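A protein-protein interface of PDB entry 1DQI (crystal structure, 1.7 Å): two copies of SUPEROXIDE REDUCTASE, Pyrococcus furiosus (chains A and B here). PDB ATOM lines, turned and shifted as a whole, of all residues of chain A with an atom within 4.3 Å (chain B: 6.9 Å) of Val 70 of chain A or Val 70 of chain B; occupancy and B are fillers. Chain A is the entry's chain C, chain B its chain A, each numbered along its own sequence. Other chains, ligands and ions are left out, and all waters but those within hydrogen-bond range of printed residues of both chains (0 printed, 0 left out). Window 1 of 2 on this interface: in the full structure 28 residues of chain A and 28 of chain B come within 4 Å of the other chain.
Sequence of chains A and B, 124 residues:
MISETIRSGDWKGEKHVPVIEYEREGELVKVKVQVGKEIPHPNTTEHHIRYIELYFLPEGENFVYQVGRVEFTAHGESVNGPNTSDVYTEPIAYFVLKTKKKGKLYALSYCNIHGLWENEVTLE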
ATOM      1  N   TYR A  51       9.121 -12.793  13.705  1.00  0.00           N
ATOM      2  CA  TYR A  51       9.306 -12.068  12.456  1.00  0.00           C
ATOM      3  C   TYR A  51      10.764 -11.778  12.150  1.00  0.00           C
ATOM      4  O   TYR A  51      11.638 -11.942  13.003  1.00  0.00           O
ATOM      5  CB  TYR A  51       8.555 -10.728  12.528  1.00  0.00           C
ATOM      6  CG  TYR A  51       9.128  -9.764  13.563  1.00  0.00           C
ATOM      7  CD1 TYR A  51      10.280  -9.021  13.295  1.00  0.00           C
ATOM      8  CD2 TYR A  51       8.525  -9.610  14.814  1.00  0.00           C
ATOM      9  CE1 TYR A  51      10.822  -8.154  14.246  1.00  0.00           C
ATOM     10  CE2 TYR A  51       9.058  -8.744  15.772  1.00  0.00           C
ATOM     11  CZ  TYR A  51      10.206  -8.021  15.479  1.00  0.00           C
ATOM     12  OH  TYR A  51      10.737  -7.172  16.425  1.00  0.00           O
ATOM     13  N   ILE A  52      11.007 -11.344  10.918  1.00  0.00           N
ATOM     14  CA  ILE A  52      12.331 -10.944  10.474  1.00  0.00           C
ATOM     15  C   ILE A  52      12.123  -9.661   9.678  1.00  0.00           C
ATOM     16  O   ILE A  52      11.213  -9.575   8.850  1.00  0.00           O
ATOM     17  CB  ILE A  52      12.990 -11.994   9.553  1.00  0.00           C
ATOM     18  CG1 ILE A  52      13.494 -13.173  10.385  1.00  0.00           C
ATOM     19  CG2 ILE A  52      14.144 -11.368   8.786  1.00  0.00           C
ATOM     20  CD1 ILE A  52      14.091 -14.295   9.537  1.00  0.00           C
ATOM     21  N   ARG A  69       9.338  -6.476   6.003  1.00  0.00           N
ATOM     22  CA  ARG A  69       9.118  -7.170   7.254  1.00  0.00           C
ATOM     23  C   ARG A  69       8.283  -8.400   6.944  1.00  0.00           C
ATOM     24  O   ARG A  69       7.300  -8.324   6.207  1.00  0.00           O
ATOM     25  CB  ARG A  69       8.382  -6.232   8.211  1.00  0.00           C
ATOM     26  CG  ARG A  69       7.624  -6.890   9.335  1.00  0.00           C
ATOM     27  CD  ARG A  69       6.826  -5.827  10.086  1.00  0.00           C
ATOM     28  NE  ARG A  69       5.955  -6.388  11.110  1.00  0.00           N
ATOM     29  CZ  ARG A  69       6.367  -6.746  12.322  1.00  0.00           C
ATOM     30  NH1 ARG A  69       7.637  -6.603  12.661  1.00  0.00           N
ATOM     31  NH2 ARG A  69       5.505  -7.244  13.196  1.00  0.00           N
ATOM     32  N   VAL A  70       8.694  -9.542   7.476  1.00  0.00           N
ATOM     33  CA  VAL A  70       7.950 -10.771   7.262  1.00  0.00           C
ATOM     34  C   VAL A  70       7.556 -11.324   8.621  1.00  0.00           C
ATOM     35  O   VAL A  70       8.414 -11.556   9.481  1.00  0.00           O
ATOM     36  CB  VAL A  70       8.793 -11.824   6.502  1.00  0.00           C
ATOM     37  CG1 VAL A  70       8.002 -13.115   6.354  1.00  0.00           C
ATOM     38  CG2 VAL A  70       9.185 -11.287   5.130  1.00  0.00           C
ATOM     39  N   GLU A  71       6.253 -11.507   8.819  1.00  0.00           N
ATOM     40  CA  GLU A  71       5.733 -12.045  10.069  1.00  0.00           C
ATOM     41  C   GLU A  71       5.327 -13.501   9.863  1.00  0.00           C
ATOM     42  O   GLU A  71       4.583 -13.818   8.933  1.00  0.00           O
ATOM     43  CB  GLU A  71       4.520 -11.233  10.534  1.00  0.00           C
ATOM     44  CG  GLU A  71       4.839  -9.778  10.837  1.00  0.00           C
ATOM     45  CD  GLU A  71       3.612  -8.967  11.203  1.00  0.00           C
ATOM     46  OE1 GLU A  71       3.771  -7.772  11.517  1.00  0.00           O
ATOM     47  OE2 GLU A  71       2.491  -9.518  11.177  1.00  0.00           O
ATOM     48  N   PHE A  72       5.848 -14.373  10.722  1.00  0.00           N
ATOM     49  CA  PHE A  72       5.548 -15.807  10.695  1.00  0.00           C
ATOM     50  C   PHE A  72       4.478 -15.946  11.773  1.00  0.00           C
ATOM     51  O   PHE A  72       4.777 -15.942  12.962  1.00  0.00           O
ATOM     52  CB  PHE A  72       6.811 -16.596  11.039  1.00  0.00           C
ATOM     53  CG  PHE A  72       8.045 -16.090  10.340  1.00  0.00           C
ATOM     54  CD1 PHE A  72       9.109 -15.575  11.070  1.00  0.00           C
ATOM     55  CD2 PHE A  72       8.136 -16.112   8.949  1.00  0.00           C
ATOM     56  CE1 PHE A  72      10.249 -15.089  10.431  1.00  0.00           C
ATOM     57  CE2 PHE A  72       9.279 -15.626   8.295  1.00  0.00           C
ATOM     58  CZ  PHE A  72      10.334 -15.115   9.040  1.00  0.00           C
ATOM     59  N   ALA A  93      12.586 -15.804   5.430  1.00  0.00           N
ATOM     60  CA  ALA A  93      12.076 -14.611   4.772  1.00  0.00           C
ATOM     61  C   ALA A  93      12.800 -14.299   3.473  1.00  0.00           C
ATOM     62  O   ALA A  93      14.027 -14.344   3.397  1.00  0.00           O
ATOM     63  CB  ALA A  93      12.176 -13.418   5.719  1.00  0.00           C
ATOM     64  N   PHE A  95      13.039 -11.425   0.282  1.00  0.00           N
ATOM     65  CA  PHE A  95      12.734 -10.052  -0.112  1.00  0.00           C
ATOM     66  C   PHE A  95      13.318  -9.787  -1.489  1.00  0.00           C
ATOM     67  O   PHE A  95      14.461 -10.149  -1.759  1.00  0.00           O
ATOM     68  CB  PHE A  95      13.362  -9.047   0.859  1.00  0.00           C
ATOM     69  CG  PHE A  95      13.009  -9.274   2.298  1.00  0.00           C
ATOM     70  CD1 PHE A  95      13.771 -10.126   3.089  1.00  0.00           C
ATOM     71  CD2 PHE A  95      11.934  -8.607   2.875  1.00  0.00           C
ATOM     72  CE1 PHE A  95      13.470 -10.312   4.440  1.00  0.00           C
ATOM     73  CE2 PHE A  95      11.624  -8.783   4.225  1.00  0.00           C
ATOM     74  CZ  PHE A  95      12.394  -9.636   5.008  1.00  0.00           C
ATOM     75  N   ARG B  50       1.405  -2.327  -0.698  1.00  0.00           N
ATOM     76  CA  ARG B  50       1.932  -2.265   0.662  1.00  0.00           C
ATOM     77  C   ARG B  50       2.282  -3.597   1.308  1.00  0.00           C
ATOM     78  O   ARG B  50       3.273  -3.701   2.033  1.00  0.00           O
ATOM     79  CB  ARG B  50       0.939  -1.537   1.569  1.00  0.00           C
ATOM     80  CG  ARG B  50       0.726  -0.071   1.210  1.00  0.00           C
ATOM     81  CD  ARG B  50       1.716   0.829   1.945  1.00  0.00           C
ATOM     82  NE  ARG B  50       1.368   2.245   1.816  1.00  0.00           N
ATOM     83  CZ  ARG B  50       0.431   2.859   2.535  1.00  0.00           C
ATOM     84  NH1 ARG B  50      -0.264   2.185   3.442  1.00  0.00           N
ATOM     85  NH2 ARG B  50       0.195   4.155   2.352  1.00  0.00           N
ATOM     86  N   TYR B  51       1.469  -4.616   1.059  1.00  0.00           N
ATOM     87  CA  TYR B  51       1.715  -5.909   1.680  1.00  0.00           C
ATOM     88  C   TYR B  51       0.870  -7.014   1.081  1.00  0.00           C
ATOM     89  O   TYR B  51      -0.081  -6.760   0.342  1.00  0.00           O
ATOM     90  CB  TYR B  51       1.393  -5.820   3.180  1.00  0.00           C
ATOM     91  CG  TYR B  51      -0.085  -5.584   3.473  1.00  0.00           C
ATOM     92  CD1 TYR B  51      -1.011  -6.624   3.389  1.00  0.00           C
ATOM     93  CD2 TYR B  51      -0.555  -4.316   3.821  1.00  0.00           C
ATOM     94  CE1 TYR B  51      -2.364  -6.413   3.643  1.00  0.00           C
ATOM     95  CE2 TYR B  51      -1.908  -4.092   4.077  1.00  0.00           C
ATOM     96  CZ  TYR B  51      -2.807  -5.147   3.986  1.00  0.00           C
ATOM     97  OH  TYR B  51      -4.145  -4.936   4.240  1.00  0.00           O
ATOM     98  N   ILE B  52       1.234  -8.246   1.422  1.00  0.00           N
ATOM     99  CA  ILE B  52       0.495  -9.425   1.005  1.00  0.00           C
ATOM    100  C   ILE B  52       0.395 -10.294   2.253  1.00  0.00           C
ATOM    101  O   ILE B  52       1.372 -10.451   2.988  1.00  0.00           O
ATOM    102  CB  ILE B  52       1.227 -10.226  -0.091  1.00  0.00           C
ATOM    103  CG1 ILE B  52       1.085  -9.519  -1.437  1.00  0.00           C
ATOM    104  CG2 ILE B  52       0.650 -11.638  -0.179  1.00  0.00           C
ATOM    105  CD1 ILE B  52       1.914 -10.158  -2.551  1.00  0.00           C
ATOM    106  N   GLU B  53      -0.793 -10.837   2.498  1.00  0.00           N
ATOM    107  CA  GLU B  53      -1.029 -11.708   3.645  1.00  0.00           C
ATOM    108  C   GLU B  53      -1.466 -13.066   3.104  1.00  0.00           C
ATOM    109  O   GLU B  53      -2.158 -13.137   2.087  1.00  0.00           O
ATOM    110  CB  GLU B  53      -2.143 -11.135   4.533  1.00  0.00           C
ATOM    111  CG  GLU B  53      -1.751  -9.892   5.309  1.00  0.00           C
ATOM    112  CD  GLU B  53      -2.914  -9.283   6.077  1.00  0.00           C
ATOM    113  OE1 GLU B  53      -4.080  -9.614   5.778  1.00  0.00           O
ATOM    114  OE2 GLU B  53      -2.659  -8.465   6.985  1.00  0.00           O
ATOM    115  N   LEU B  54      -1.054 -14.139   3.773  1.00  0.00           N
ATOM    116  CA  LEU B  54      -1.431 -15.485   3.353  1.00  0.00           C
ATOM    117  C   LEU B  54      -2.200 -16.173   4.473  1.00  0.00           C
ATOM    118  O   LEU B  54      -1.791 -16.132   5.635  1.00  0.00           O
ATOM    119  CB  LEU B  54      -0.191 -16.314   2.993  1.00  0.00           C
ATOM    120  CG  LEU B  54      -0.491 -17.748   2.528  1.00  0.00           C
ATOM    121  CD1 LEU B  54      -1.119 -17.722   1.138  1.00  0.00           C
ATOM    122  CD2 LEU B  54       0.787 -18.571   2.511  1.00  0.00           C
ATOM    123  N   GLY B  68       1.115 -15.947   7.310  1.00  0.00           N
ATOM    124  CA  GLY B  68       2.128 -14.920   7.405  1.00  0.00           C
ATOM    125  C   GLY B  68       1.712 -13.626   6.751  1.00  0.00           C
ATOM    126  O   GLY B  68       0.656 -13.529   6.128  1.00  0.00           O
ATOM    127  N   ARG B  69       2.562 -12.624   6.915  1.00  0.00           N
ATOM    128  CA  ARG B  69       2.327 -11.313   6.354  1.00  0.00           C
ATOM    129  C   ARG B  69       3.670 -10.771   5.898  1.00  0.00           C
ATOM    130  O   ARG B  69       4.669 -10.890   6.605  1.00  0.00           O
ATOM    131  CB  ARG B  69       1.713 -10.421   7.430  1.00  0.00           C
ATOM    132  CG  ARG B  69       1.708  -8.950   7.140  1.00  0.00           C
ATOM    133  CD  ARG B  69       1.034  -8.227   8.297  1.00  0.00           C
ATOM    134  NE  ARG B  69       1.349  -6.806   8.319  1.00  0.00           N
ATOM    135  CZ  ARG B  69       0.687  -5.890   7.624  1.00  0.00           C
ATOM    136  NH1 ARG B  69      -0.326  -6.247   6.852  1.00  0.00           N
ATOM    137  NH2 ARG B  69       1.040  -4.615   7.693  1.00  0.00           N
ATOM    138  N   VAL B  70       3.704 -10.211   4.696  1.00  0.00           N
ATOM    139  CA  VAL B  70       4.931  -9.633   4.178  1.00  0.00           C
ATOM    140  C   VAL B  70       4.639  -8.191   3.805  1.00  0.00           C
ATOM    141  O   VAL B  70       3.746  -7.921   2.997  1.00  0.00           O
ATOM    142  CB  VAL B  70       5.444 -10.388   2.927  1.00  0.00           C
ATOM    143  CG1 VAL B  70       6.715  -9.727   2.410  1.00  0.00           C
ATOM    144  CG2 VAL B  70       5.714 -11.841   3.268  1.00  0.00           C
ATOM    145  N   GLU B  71       5.376  -7.271   4.419  1.00  0.00           N
ATOM    146  CA  GLU B  71       5.218  -5.852   4.152  1.00  0.00           C
ATOM    147  C   GLU B  71       6.366  -5.384   3.262  1.00  0.00           C
ATOM    148  O   GLU B  71       7.538  -5.638   3.558  1.00  0.00           O
ATOM    149  CB  GLU B  71       5.221  -5.060   5.466  1.00  0.00           C
ATOM    150  CG  GLU B  71       4.134  -5.499   6.438  1.00  0.00           C
ATOM    151  CD  GLU B  71       4.156  -4.734   7.750  1.00  0.00           C
ATOM    152  OE1 GLU B  71       3.251  -4.963   8.575  1.00  0.00           O
ATOM    153  OE2 GLU B  71       5.070  -3.909   7.961  1.00  0.00           O
ATOM    154  N   PHE B  72       6.017  -4.727   2.159  1.00  0.00           N
ATOM    155  CA  PHE B  72       6.996  -4.190   1.213  1.00  0.00           C
ATOM    156  C   PHE B  72       7.059  -2.722   1.610  1.00  0.00           C
ATOM    157  O   PHE B  72       6.160  -1.939   1.302  1.00  0.00           O
ATOM    158  CB  PHE B  72       6.479  -4.374  -0.216  1.00  0.00           C
ATOM    159  CG  PHE B  72       5.897  -5.740  -0.474  1.00  0.00           C
ATOM    160  CD1 PHE B  72       4.550  -5.891  -0.790  1.00  0.00           C
ATOM    161  CD2 PHE B  72       6.692  -6.881  -0.372  1.00  0.00           C
ATOM    162  CE1 PHE B  72       4.001  -7.162  -0.998  1.00  0.00           C
ATOM    163  CE2 PHE B  72       6.149  -8.157  -0.579  1.00  0.00           C
ATOM    164  CZ  PHE B  72       4.804  -8.294  -0.892  1.00  0.00           C
ATOM    165  N   THR B  89      10.894  -2.093  -2.868  1.00  0.00           N
ATOM    166  CA  THR B  89      10.629  -3.479  -2.504  1.00  0.00           C
ATOM    167  C   THR B  89       9.504  -4.002  -3.385  1.00  0.00           C
ATOM    168  O   THR B  89       8.385  -3.493  -3.353  1.00  0.00           O
ATOM    169  CB  THR B  89      10.220  -3.595  -1.030  1.00  0.00           C
ATOM    170  OG1 THR B  89      11.161  -2.877  -0.225  1.00  0.00           O
ATOM    171  CG2 THR B  89      10.205  -5.058  -0.595  1.00  0.00           C
ATOM    172  N   GLU B  90       9.811  -5.018  -4.183  1.00  0.00           N
ATOM    173  CA  GLU B  90       8.829  -5.596  -5.094  1.00  0.00           C
ATOM    174  C   GLU B  90       7.801  -6.440  -4.358  1.00  0.00           C
ATOM    175  O   GLU B  90       8.131  -7.128  -3.396  1.00  0.00           O
ATOM    176  CB  GLU B  90       9.549  -6.440  -6.146  1.00  0.00           C
ATOM    177  CG  GLU B  90      10.399  -5.609  -7.087  1.00  0.00           C
ATOM    178  CD  GLU B  90       9.559  -4.709  -7.970  1.00  0.00           C
ATOM    179  OE1 GLU B  90       9.231  -5.133  -9.097  1.00  0.00           O
ATOM    180  OE2 GLU B  90       9.220  -3.585  -7.538  1.00  0.00           O
ATOM    181  N   ILE B  92       6.537  -9.319  -4.018  1.00  0.00           N
ATOM    182  CA  ILE B  92       6.693 -10.755  -4.193  1.00  0.00           C
ATOM    183  C   ILE B  92       6.866 -11.327  -2.795  1.00  0.00           C
ATOM    184  O   ILE B  92       7.786 -10.944  -2.071  1.00  0.00           O
ATOM    185  CB  ILE B  92       7.933 -11.095  -5.041  1.00  0.00           C
ATOM    186  CG1 ILE B  92       7.750 -10.570  -6.463  1.00  0.00           C
ATOM    187  CG2 ILE B  92       8.147 -12.602  -5.071  1.00  0.00           C
ATOM    188  CD1 ILE B  92       9.049 -10.411  -7.227  1.00  0.00           C
ATOM    189  N   ALA B  93       5.972 -12.231  -2.415  1.00  0.00           N
ATOM    190  CA  ALA B  93       6.016 -12.834  -1.095  1.00  0.00           C
ATOM    191  C   ALA B  93       6.200 -14.342  -1.159  1.00  0.00           C
ATOM    192  O   ALA B  93       5.600 -15.025  -1.988  1.00  0.00           O
ATOM    193  CB  ALA B  93       4.740 -12.498  -0.329  1.00  0.00           C
ATOM    194  N   TYR B  94       7.044 -14.853  -0.275  1.00  0.00           N
ATOM    195  CA  TYR B  94       7.303 -16.278  -0.206  1.00  0.00           C
ATOM    196  C   TYR B  94       7.065 -16.709   1.232  1.00  0.00           C
ATOM    197  O   TYR B  94       7.486 -16.027   2.168  1.00  0.00           O
ATOM    198  CB  TYR B  94       8.747 -16.567  -0.606  1.00  0.00           C
ATOM    199  CG  TYR B  94       9.004 -17.997  -1.015  1.00  0.00           C
ATOM    200  CD1 TYR B  94       8.823 -18.408  -2.335  1.00  0.00           C
ATOM    201  CD2 TYR B  94       9.458 -18.935  -0.088  1.00  0.00           C
ATOM    202  CE1 TYR B  94       9.093 -19.718  -2.725  1.00  0.00           C
ATOM    203  CE2 TYR B  94       9.730 -20.249  -0.467  1.00  0.00           C
ATOM    204  CZ  TYR B  94       9.546 -20.631  -1.787  1.00  0.00           C
ATOM    205  OH  TYR B  94       9.833 -21.918  -2.176  1.00  0.00           O
ATOM    206  N   PHE B  95       6.369 -17.826   1.403  1.00  0.00           N
ATOM    207  CA  PHE B  95       6.076 -18.350   2.728  1.00  0.00           C
ATOM    208  C   PHE B  95       6.414 -19.829   2.756  1.00  0.00           C
ATOM    209  O   PHE B  95       6.089 -20.560   1.822  1.00  0.00           O
ATOM    210  CB  PHE B  95       4.588 -18.190   3.060  1.00  0.00           C
ATOM    211  CG  PHE B  95       4.068 -16.791   2.889  1.00  0.00           C
ATOM    212  CD1 PHE B  95       3.654 -16.337   1.642  1.00  0.00           C
ATOM    213  CD2 PHE B  95       3.967 -15.938   3.981  1.00  0.00           C
ATOM    214  CE1 PHE B  95       3.144 -15.052   1.482  1.00  0.00           C
ATOM    215  CE2 PHE B  95       3.460 -14.649   3.835  1.00  0.00           C
ATOM    216  CZ  PHE B  95       3.047 -14.205   2.583  1.00  0.00           C
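N of Glu 71 of chain A sits at hydrogen-bond distance from O of Arg 69 of chain B (2.8 Å).
OE1 of Glu 71 of chain B lies within salt-bridge range of NE of Arg 69 of chain A (3.97 Å).
O of Ile 52 of chain B sits at hydrogen-bond distance from N of Val 70 of chain B, at 2.9 Å.
OE2 of Glu 53 of chain B is in salt-bridge range of NH1 of Arg 69 of chain B (3.2 Å).
The backbone carbonyl oxygen (O) of Gly 68 of chain B lies within hydrogen-bond range of the backbone NH (N) of Leu 54 of chain B (3.0 Å).
The side-chain carboxylate (OE1) of Glu 71 of chain B lies within salt-bridge range of the guanidinium group (NH2) of Arg 69 of chain B, at 2.4 Å.
N of Val 70 of chain A sits at hydrogen-bond distance from O of Ile 52 of chain A, at 2.9 Å.
The guanidinium group (NH2) of Arg 69 of chain A lies within salt-bridge range of the side-chain carboxylate (OE1) of Glu 71 of chain A (2.5 Å).
Among the printed residues, merely in contact across the chains: Arg 69 of chain A with Arg 69 of chain B, Arg 69 of chain A with Val 70 of chain B, Val 70 of chain A with Arg 69 of chain B, Val 70 of chain A with Val 70 of chain B and Glu 71 of chain A with Gly 68 of chain B.
Of the printed residues of chain B, Val 70 of chain A touches Arg 69 (3.3 Å) and Val 70 (3.98 Å).
Of chain A, only Arg 69 and Val 70 come within 4 Å of Val 70 of chain B.
Printed residues of chain A within 4 Å of Gly 68 of chain B: Glu 71.
Printed residues of chain B within 4 Å of Arg 69 of chain A: Arg 69 (3.7 Å), Val 70 (3.4 Å) and Glu 71 (2.8 Å).
Of the printed residues of chain B, Glu 71 of chain A touches Gly 68 and Arg 69.
Printed residues of chain A within 4 Å of Glu 71 of chain B: Arg 69.
Tyr 94 of chain B touches none of the printed residues of chain A.
Thr 89 of chain B touches none of the printed residues of chain A.
The nearest printed residue of chain A that does not touch Val 70 of chain B is Glu 71 of chain A (5.0 Å).
Hydrophobic or aromatic side chains of chain B within 4 Å of the printed part of chain A: Val 70.
Of the 8 printed residues of chain A, 3 touch a printed residue of chain B.
Hydrophobic or aromatic side chains of chain A that line the printed part of chain B: Val 70.
Along chain A the printed residues that touch a printed residue of chain B span positions 69 to 71.
Among the printed residues, Asp or Glu carboxylates within 4 Å of a Lys or Arg side-chain nitrogen of the other chain: Arg 69 of chain A with Glu 71 of chain B.
Arg 69 of chain A touches its own counterpart, Arg 69 of chain B.
Arg 69 of chain A touches Val 70 of chain B, and with the chains exchanged Val 70 of chain A touches Arg 69 of chain B.
Arg 69 of chain A touches Glu 71 of chain B, and with the chains exchanged Glu 71 of chain A touches Arg 69 of chain B.
Val 70 of chain A touches its own counterpart, Val 70 of chain B.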
